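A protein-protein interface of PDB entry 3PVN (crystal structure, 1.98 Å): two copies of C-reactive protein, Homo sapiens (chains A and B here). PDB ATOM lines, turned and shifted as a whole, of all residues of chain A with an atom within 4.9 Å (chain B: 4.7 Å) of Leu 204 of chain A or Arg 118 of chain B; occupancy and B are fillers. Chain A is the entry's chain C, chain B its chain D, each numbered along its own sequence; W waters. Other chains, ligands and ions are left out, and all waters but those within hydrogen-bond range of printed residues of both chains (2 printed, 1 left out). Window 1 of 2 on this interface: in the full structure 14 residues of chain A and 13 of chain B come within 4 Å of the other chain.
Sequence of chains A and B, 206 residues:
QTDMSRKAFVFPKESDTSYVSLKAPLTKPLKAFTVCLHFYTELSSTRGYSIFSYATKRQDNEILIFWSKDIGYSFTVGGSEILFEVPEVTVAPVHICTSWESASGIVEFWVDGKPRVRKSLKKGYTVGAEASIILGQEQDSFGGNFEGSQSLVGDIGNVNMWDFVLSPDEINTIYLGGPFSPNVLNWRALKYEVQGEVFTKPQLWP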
ATOM      1  N   VAL A  10      22.397 -12.697  21.034  1.00  0.00           N
ATOM      2  CA  VAL A  10      23.323 -13.840  21.256  1.00  0.00           C
ATOM      3  C   VAL A  10      24.570 -13.616  20.405  1.00  0.00           C
ATOM      4  O   VAL A  10      24.468 -13.423  19.160  1.00  0.00           O
ATOM      5  CB  VAL A  10      22.718 -15.184  20.864  1.00  0.00           C
ATOM      6  CG1 VAL A  10      23.700 -16.410  21.285  1.00  0.00           C
ATOM      7  CG2 VAL A  10      21.390 -15.411  21.579  1.00  0.00           C
ATOM      8  N   PRO A  12      27.628 -15.815  19.842  1.00  0.00           N
ATOM      9  CA  PRO A  12      28.021 -17.230  20.090  1.00  0.00           C
ATOM     10  C   PRO A  12      29.511 -17.528  20.005  1.00  0.00           C
ATOM     11  O   PRO A  12      29.895 -18.620  20.351  1.00  0.00           O
ATOM     12  CB  PRO A  12      27.349 -18.004  18.971  1.00  0.00           C
ATOM     13  CG  PRO A  12      26.615 -17.011  18.116  1.00  0.00           C
ATOM     14  CD  PRO A  12      26.866 -15.653  18.584  1.00  0.00           C
ATOM     15  N   TYR A  40      24.691 -13.167  30.309  1.00  0.00           N
ATOM     16  CA  TYR A  40      25.109 -14.493  30.683  1.00  0.00           C
ATOM     17  C   TYR A  40      26.293 -14.896  29.793  1.00  0.00           C
ATOM     18  O   TYR A  40      26.161 -14.966  28.525  1.00  0.00           O
ATOM     19  CB  TYR A  40      23.939 -15.445  30.443  1.00  0.00           C
ATOM     20  CG  TYR A  40      24.162 -16.861  31.001  1.00  0.00           C
ATOM     21  CD1 TYR A  40      25.109 -17.100  32.059  1.00  0.00           C
ATOM     22  CD2 TYR A  40      23.463 -17.953  30.463  1.00  0.00           C
ATOM     23  CE1 TYR A  40      25.300 -18.343  32.590  1.00  0.00           C
ATOM     24  CE2 TYR A  40      23.649 -19.245  30.992  1.00  0.00           C
ATOM     25  CZ  TYR A  40      24.565 -19.444  32.021  1.00  0.00           C
ATOM     26  OH  TYR A  40      24.713 -20.734  32.505  1.00  0.00           O
ATOM     27  N   ASP A 155      25.095 -14.050  26.002  1.00  0.00           N
ATOM     28  CA  ASP A 155      23.814 -13.381  25.730  1.00  0.00           C
ATOM     29  C   ASP A 155      23.719 -12.119  26.552  1.00  0.00           C
ATOM     30  O   ASP A 155      24.244 -12.033  27.689  1.00  0.00           O
ATOM     31  CB  ASP A 155      22.646 -14.236  26.211  1.00  0.00           C
ATOM     32  CG  ASP A 155      22.388 -15.481  25.376  1.00  0.00           C
ATOM     33  OD1 ASP A 155      23.303 -16.016  24.700  1.00  0.00           O
ATOM     34  OD2 ASP A 155      21.215 -15.992  25.443  1.00  0.00           O
ATOM     35  N   LYS A 201      17.214 -14.278  20.044  1.00  0.00           N
ATOM     36  CA  LYS A 201      16.641 -15.542  20.472  1.00  0.00           C
ATOM     37  C   LYS A 201      15.847 -15.326  21.755  1.00  0.00           C
ATOM     38  O   LYS A 201      16.075 -14.407  22.449  1.00  0.00           O
ATOM     39  CB  LYS A 201      17.818 -16.541  20.798  1.00  0.00           C
ATOM     40  CG  LYS A 201      18.620 -17.067  19.498  1.00  0.00           C
ATOM     41  CD  LYS A 201      17.689 -17.874  18.616  1.00  0.00           C
ATOM     42  CE  LYS A 201      18.290 -18.280  17.270  1.00  0.00           C
ATOM     43  NZ  LYS A 201      17.293 -19.088  16.471  1.00  0.00           N
ATOM     44  N   PRO A 202      15.008 -16.258  22.137  1.00  0.00           N
ATOM     45  CA  PRO A 202      14.313 -16.055  23.408  1.00  0.00           C
ATOM     46  C   PRO A 202      15.316 -16.090  24.545  1.00  0.00           C
ATOM     47  O   PRO A 202      16.277 -16.950  24.511  1.00  0.00           O
ATOM     48  CB  PRO A 202      13.419 -17.284  23.531  1.00  0.00           C
ATOM     49  CG  PRO A 202      13.273 -17.819  22.180  1.00  0.00           C
ATOM     50  CD  PRO A 202      14.479 -17.373  21.359  1.00  0.00           C
ATOM     51  N   GLN A 203      15.088 -15.237  25.553  1.00  0.00           N
ATOM     52  CA  GLN A 203      15.980 -15.136  26.679  1.00  0.00           C
ATOM     53  C   GLN A 203      16.050 -16.458  27.487  1.00  0.00           C
ATOM     54  O   GLN A 203      15.068 -17.168  27.650  1.00  0.00           O
ATOM     55  CB  GLN A 203      15.586 -13.988  27.624  1.00  0.00           C
ATOM     56  CG  GLN A 203      14.351 -14.253  28.412  1.00  0.00           C
ATOM     57  CD  GLN A 203      13.838 -12.985  29.149  1.00  0.00           C
ATOM     58  OE1 GLN A 203      13.180 -13.117  30.167  1.00  0.00           O
ATOM     59  NE2 GLN A 203      14.191 -11.783  28.664  1.00  0.00           N
ATOM     60  N   LEU A 204      17.250 -16.738  27.980  1.00  0.00           N
ATOM     61  CA  LEU A 204      17.534 -17.923  28.786  1.00  0.00           C
ATOM     62  C   LEU A 204      17.140 -17.701  30.246  1.00  0.00           C
ATOM     63  O   LEU A 204      16.929 -18.670  30.964  1.00  0.00           O
ATOM     64  CB  LEU A 204      19.028 -18.231  28.744  1.00  0.00           C
ATOM     65  CG  LEU A 204      19.576 -18.695  27.419  1.00  0.00           C
ATOM     66  CD1 LEU A 204      21.087 -19.010  27.461  1.00  0.00           C
ATOM     67  CD2 LEU A 204      18.887 -19.895  27.048  1.00  0.00           C
ATOM     68  N   TRP A 205      17.080 -16.444  30.686  1.00  0.00           N
ATOM     69  CA  TRP A 205      16.754 -16.125  32.097  1.00  0.00           C
ATOM     70  C   TRP A 205      15.243 -15.913  32.296  1.00  0.00           C
ATOM     71  O   TRP A 205      14.519 -15.444  31.358  1.00  0.00           O
ATOM     72  CB  TRP A 205      17.550 -14.900  32.583  1.00  0.00           C
ATOM     73  CG  TRP A 205      17.606 -13.781  31.562  1.00  0.00           C
ATOM     74  CD1 TRP A 205      16.608 -12.888  31.272  1.00  0.00           C
ATOM     75  CD2 TRP A 205      18.680 -13.504  30.644  1.00  0.00           C
ATOM     76  NE1 TRP A 205      17.018 -12.037  30.272  1.00  0.00           N
ATOM     77  CE2 TRP A 205      18.276 -12.411  29.853  1.00  0.00           C
ATOM     78  CE3 TRP A 205      19.956 -14.079  30.414  1.00  0.00           C
ATOM     79  CZ2 TRP A 205      19.106 -11.857  28.859  1.00  0.00           C
ATOM     80  CZ3 TRP A 205      20.807 -13.494  29.468  1.00  0.00           C
ATOM     81  CH2 TRP A 205      20.355 -12.401  28.683  1.00  0.00           C
ATOM     82  N   PRO A 206      14.754 -16.229  33.504  1.00  0.00           N
ATOM     83  CA  PRO A 206      13.285 -16.165  33.595  1.00  0.00           C
ATOM     84  C   PRO A 206      12.883 -14.756  33.982  1.00  0.00           C
ATOM     85  O   PRO A 206      12.572 -14.605  35.176  1.00  0.00           O
ATOM     86  CB  PRO A 206      12.951 -17.167  34.726  1.00  0.00           C
ATOM     87  CG  PRO A 206      14.267 -17.347  35.542  1.00  0.00           C
ATOM     88  CD  PRO A 206      15.395 -16.628  34.784  1.00  0.00           C
ATOM     89  OXT PRO A 206      12.944 -13.775  33.205  1.00  0.00           O
ATOM     90  N   ILE B 106      23.843 -22.273  16.502  1.00  0.00           N
ATOM     91  CA  ILE B 106      23.695 -22.142  17.970  1.00  0.00           C
ATOM     92  C   ILE B 106      23.451 -23.497  18.633  1.00  0.00           C
ATOM     93  O   ILE B 106      22.554 -24.250  18.223  1.00  0.00           O
ATOM     94  CB  ILE B 106      22.642 -21.044  18.415  1.00  0.00           C
ATOM     95  CG1 ILE B 106      23.157 -19.646  18.090  1.00  0.00           C
ATOM     96  CG2 ILE B 106      22.285 -21.180  19.896  1.00  0.00           C
ATOM     97  CD1 ILE B 106      22.061 -18.495  18.243  1.00  0.00           C
ATOM     98  N   VAL B 107      24.250 -23.778  19.664  1.00  0.00           N
ATOM     99  CA  VAL B 107      24.041 -24.935  20.504  1.00  0.00           C
ATOM    100  C   VAL B 107      23.604 -24.499  21.926  1.00  0.00           C
ATOM    101  O   VAL B 107      24.186 -23.594  22.474  1.00  0.00           O
ATOM    102  CB  VAL B 107      25.234 -25.989  20.495  1.00  0.00           C
ATOM    103  CG1 VAL B 107      25.424 -26.559  19.112  1.00  0.00           C
ATOM    104  CG2 VAL B 107      26.590 -25.415  20.856  1.00  0.00           C
ATOM    105  N   GLU B 108      22.603 -25.161  22.512  1.00  0.00           N
ATOM    106  CA  GLU B 108      22.288 -25.020  23.918  1.00  0.00           C
ATOM    107  C   GLU B 108      22.468 -26.378  24.642  1.00  0.00           C
ATOM    108  O   GLU B 108      22.303 -27.422  24.068  1.00  0.00           O
ATOM    109  CB  GLU B 108      20.783 -24.642  24.097  1.00  0.00           C
ATOM    110  CG  GLU B 108      20.476 -23.366  23.427  1.00  0.00           C
ATOM    111  CD  GLU B 108      19.050 -22.882  23.633  1.00  0.00           C
ATOM    112  OE1 GLU B 108      18.223 -23.581  24.302  1.00  0.00           O
ATOM    113  OE2 GLU B 108      18.788 -21.812  23.057  1.00  0.00           O
ATOM    114  N   TRP B 110      21.392 -27.850  28.550  1.00  0.00           N
ATOM    115  CA  TRP B 110      20.658 -27.500  29.767  1.00  0.00           C
ATOM    116  C   TRP B 110      20.866 -28.687  30.696  1.00  0.00           C
ATOM    117  O   TRP B 110      20.716 -29.819  30.269  1.00  0.00           O
ATOM    118  CB  TRP B 110      19.167 -27.488  29.453  1.00  0.00           C
ATOM    119  CG  TRP B 110      18.713 -26.318  28.599  1.00  0.00           C
ATOM    120  CD1 TRP B 110      18.948 -26.087  27.240  1.00  0.00           C
ATOM    121  CD2 TRP B 110      17.958 -25.230  29.069  1.00  0.00           C
ATOM    122  NE1 TRP B 110      18.344 -24.867  26.847  1.00  0.00           N
ATOM    123  CE2 TRP B 110      17.741 -24.331  27.962  1.00  0.00           C
ATOM    124  CE3 TRP B 110      17.402 -24.930  30.315  1.00  0.00           C
ATOM    125  CZ2 TRP B 110      16.930 -23.203  28.068  1.00  0.00           C
ATOM    126  CZ3 TRP B 110      16.619 -23.728  30.440  1.00  0.00           C
ATOM    127  CH2 TRP B 110      16.441 -22.870  29.315  1.00  0.00           C
ATOM    128  N   PRO B 115      20.108 -23.558  32.105  1.00  0.00           N
ATOM    129  CA  PRO B 115      20.870 -23.458  30.817  1.00  0.00           C
ATOM    130  C   PRO B 115      22.339 -23.134  31.057  1.00  0.00           C
ATOM    131  O   PRO B 115      22.660 -22.417  31.973  1.00  0.00           O
ATOM    132  CB  PRO B 115      20.211 -22.248  30.111  1.00  0.00           C
ATOM    133  CG  PRO B 115      19.652 -21.420  31.266  1.00  0.00           C
ATOM    134  CD  PRO B 115      19.156 -22.417  32.296  1.00  0.00           C
ATOM    135  N   ARG B 116      23.204 -23.728  30.248  1.00  0.00           N
ATOM    136  CA  ARG B 116      24.602 -23.325  30.075  1.00  0.00           C
ATOM    137  C   ARG B 116      24.538 -22.161  29.074  1.00  0.00           C
ATOM    138  O   ARG B 116      23.464 -21.802  28.577  1.00  0.00           O
ATOM    139  CB  ARG B 116      25.464 -24.468  29.487  1.00  0.00           C
ATOM    140  CG  ARG B 116      25.661 -25.738  30.356  1.00  0.00           C
ATOM    141  CD  ARG B 116      26.303 -25.408  31.708  1.00  0.00           C
ATOM    142  NE  ARG B 116      27.674 -24.958  31.451  1.00  0.00           N
ATOM    143  CZ  ARG B 116      28.767 -25.668  31.698  1.00  0.00           C
ATOM    144  NH1 ARG B 116      28.658 -26.841  32.279  1.00  0.00           N
ATOM    145  NH2 ARG B 116      29.964 -25.196  31.341  1.00  0.00           N
ATOM    146  N   VAL B 117      25.656 -21.500  28.864  1.00  0.00           N
ATOM    147  CA  VAL B 117      25.684 -20.417  27.872  1.00  0.00           C
ATOM    148  C   VAL B 117      25.479 -21.016  26.471  1.00  0.00           C
ATOM    149  O   VAL B 117      25.860 -22.183  26.204  1.00  0.00           O
ATOM    150  CB  VAL B 117      27.024 -19.583  28.017  1.00  0.00           C
ATOM    151  CG1 VAL B 117      27.147 -18.430  26.976  1.00  0.00           C
ATOM    152  CG2 VAL B 117      27.069 -18.911  29.362  1.00  0.00           C
ATOM    153  N   ARG B 118      24.938 -20.229  25.540  1.00  0.00           N
ATOM    154  CA  ARG B 118      24.835 -20.643  24.139  1.00  0.00           C
ATOM    155  C   ARG B 118      26.217 -20.660  23.480  1.00  0.00           C
ATOM    156  O   ARG B 118      27.006 -19.794  23.748  1.00  0.00           O
ATOM    157  CB  ARG B 118      23.914 -19.655  23.378  1.00  0.00           C
ATOM    158  CG  ARG B 118      22.411 -20.027  23.716  1.00  0.00           C
ATOM    159  CD  ARG B 118      21.418 -18.906  23.248  1.00  0.00           C
ATOM    160  NE  ARG B 118      20.040 -19.363  23.350  1.00  0.00           N
ATOM    161  CZ  ARG B 118      19.022 -18.598  23.747  1.00  0.00           C
ATOM    162  NH1 ARG B 118      19.260 -17.349  24.061  1.00  0.00           N
ATOM    163  NH2 ARG B 118      17.753 -19.071  23.747  1.00  0.00           N
ATOM    164  N   LYS B 119      26.506 -21.641  22.628  1.00  0.00           N
ATOM    165  CA  LYS B 119      27.798 -21.693  21.942  1.00  0.00           C
ATOM    166  C   LYS B 119      27.547 -21.889  20.428  1.00  0.00           C
ATOM    167  O   LYS B 119      26.369 -21.975  20.015  1.00  0.00           O
ATOM    168  CB  LYS B 119      28.670 -22.812  22.545  1.00  0.00           C
ATOM    169  CG  LYS B 119      29.035 -22.490  24.011  1.00  0.00           C
ATOM    170  CD  LYS B 119      30.106 -23.516  24.584  1.00  0.00           C
ATOM    171  CE  LYS B 119      30.520 -22.994  25.971  1.00  0.00           C
ATOM    172  NZ  LYS B 119      31.645 -23.805  26.580  1.00  0.00           N
ATOM    173  N   PRO B 168      13.175 -21.999  25.604  1.00  0.00           N
ATOM    174  CA  PRO B 168      13.469 -22.158  27.022  1.00  0.00           C
ATOM    175  C   PRO B 168      12.235 -22.501  27.847  1.00  0.00           C
ATOM    176  O   PRO B 168      12.350 -23.214  28.837  1.00  0.00           O
ATOM    177  CB  PRO B 168      14.056 -20.787  27.417  1.00  0.00           C
ATOM    178  CG  PRO B 168      14.671 -20.326  26.195  1.00  0.00           C
ATOM    179  CD  PRO B 168      13.689 -20.726  25.094  1.00  0.00           C
HETATM  180  O   HOH W   1      21.886 -21.203  34.225  1.00  0.00           O
HETATM  181  O   HOH W   2      24.301 -17.560  26.531  1.00  0.00           O
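OH of Tyr 40 of chain A lies within hydrogen-bond range of O of Pro 115 of chain B.
The side-chain carboxylate (OD2) of Asp 155 of chain A lies within salt-bridge range of the guanidinium group (NH1) of Arg 118 of chain B (2.8 Å).
The backbone carbonyl oxygen of Pro 202 of chain A is in hydrogen-bond range of the guanidinium group of Arg 118 of chain B (2.7 Å).
N of Asp 155 of chain A sits at hydrogen-bond distance from O of Tyr 40 of chain A (2.9 Å).
OE1 of Gln 203 of chain A lies close to O of Trp 205 of chain A.
OE1 of Gln 203 of chain A lies close to OXT of Pro 206 of chain A, at 3.1 Å.
OE1 of Glu 108 of chain B lies within hydrogen-bond range of NE1 of Trp 110 of chain B (2.9 Å).
NE of Arg 118 of chain B is in salt-bridge range of OE2 of Glu 108 of chain B.
Val 10 of chain A touches Arg 118 of chain B.
CE2 of Tyr 40 of chain A touches O of Arg 116 of chain B, at 3.5 Å.
Tyr 40 of chain A touches Val 117 of chain B (CZ to CG2, 3.7 Å).
Lys 201 of chain A touches Ile 106 of chain B.
Lys 201 of chain A touches Arg 118 of chain B (CB to NH1, 3.7 Å).
CB of Pro 202 of chain A touches CD of Pro 168 of chain B, 3.8 Å away.
Gln 203 of chain A touches Pro 168 of chain B.
CZ2 of Trp 110 of chain B touches CD2 of Leu 204 of chain A (3.98 Å).
O of Leu 204 of chain A touches CG of Pro 115 of chain B (3.9 Å).
Leu 204 of chain A touches Arg 116 of chain B.
Leu 204 of chain A touches just these residues of chain B: Trp 110 (3.98 Å), Pro 115 (3.9 Å), Arg 116 (3.8 Å) and Arg 118 (3.5 Å).
Arg 118 of chain B touches five residues of chain A.
Printed residues of chain B within 4 Å of Lys 201 of chain A: Ile 106 and Arg 118.
Printed residues of chain A within 4 Å of Trp 110 of chain B: Leu 204.
Trp 205 of chain A touches none of the printed residues of chain B.
Glu 108 of chain B touches none of the printed residues of chain A.
The nearest residue of chain B that does not touch Leu 204 of chain A is Pro 168 of chain B (4.3 Å).
Printed residues of chain B that touch a printed residue of chain A: Ile 106, Trp 110, Pro 115, Arg 116, Val 117, Arg 118 and Pro 168.
Along chain B the printed residues that touch a printed residue of chain A span positions 106 to 168.
Hydrophobic or aromatic side chains of chain A within 4 Å of the printed part of chain B: Val 10, Tyr 40, Pro 202 and Leu 204.
Among the printed residues, Asp or Glu carboxylates within 4 Å of a Lys or Arg side-chain nitrogen of the other chain: Asp 155 of chain A with Arg 118 of chain B (2.8 Å).
No position is printed for both chains.
Of the 14 pairs that touch across the chains among the printed residues, none has its exchanged pair printed and touching as well.
Water W2 bridges the side-chain carboxylate of Asp 155 of chain A and the backbone NH of Arg 118 of chain B.
Water W1 lies within hydrogen-bond range of O of Pro 115 of chain B and OH of Tyr 40 of chain A.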
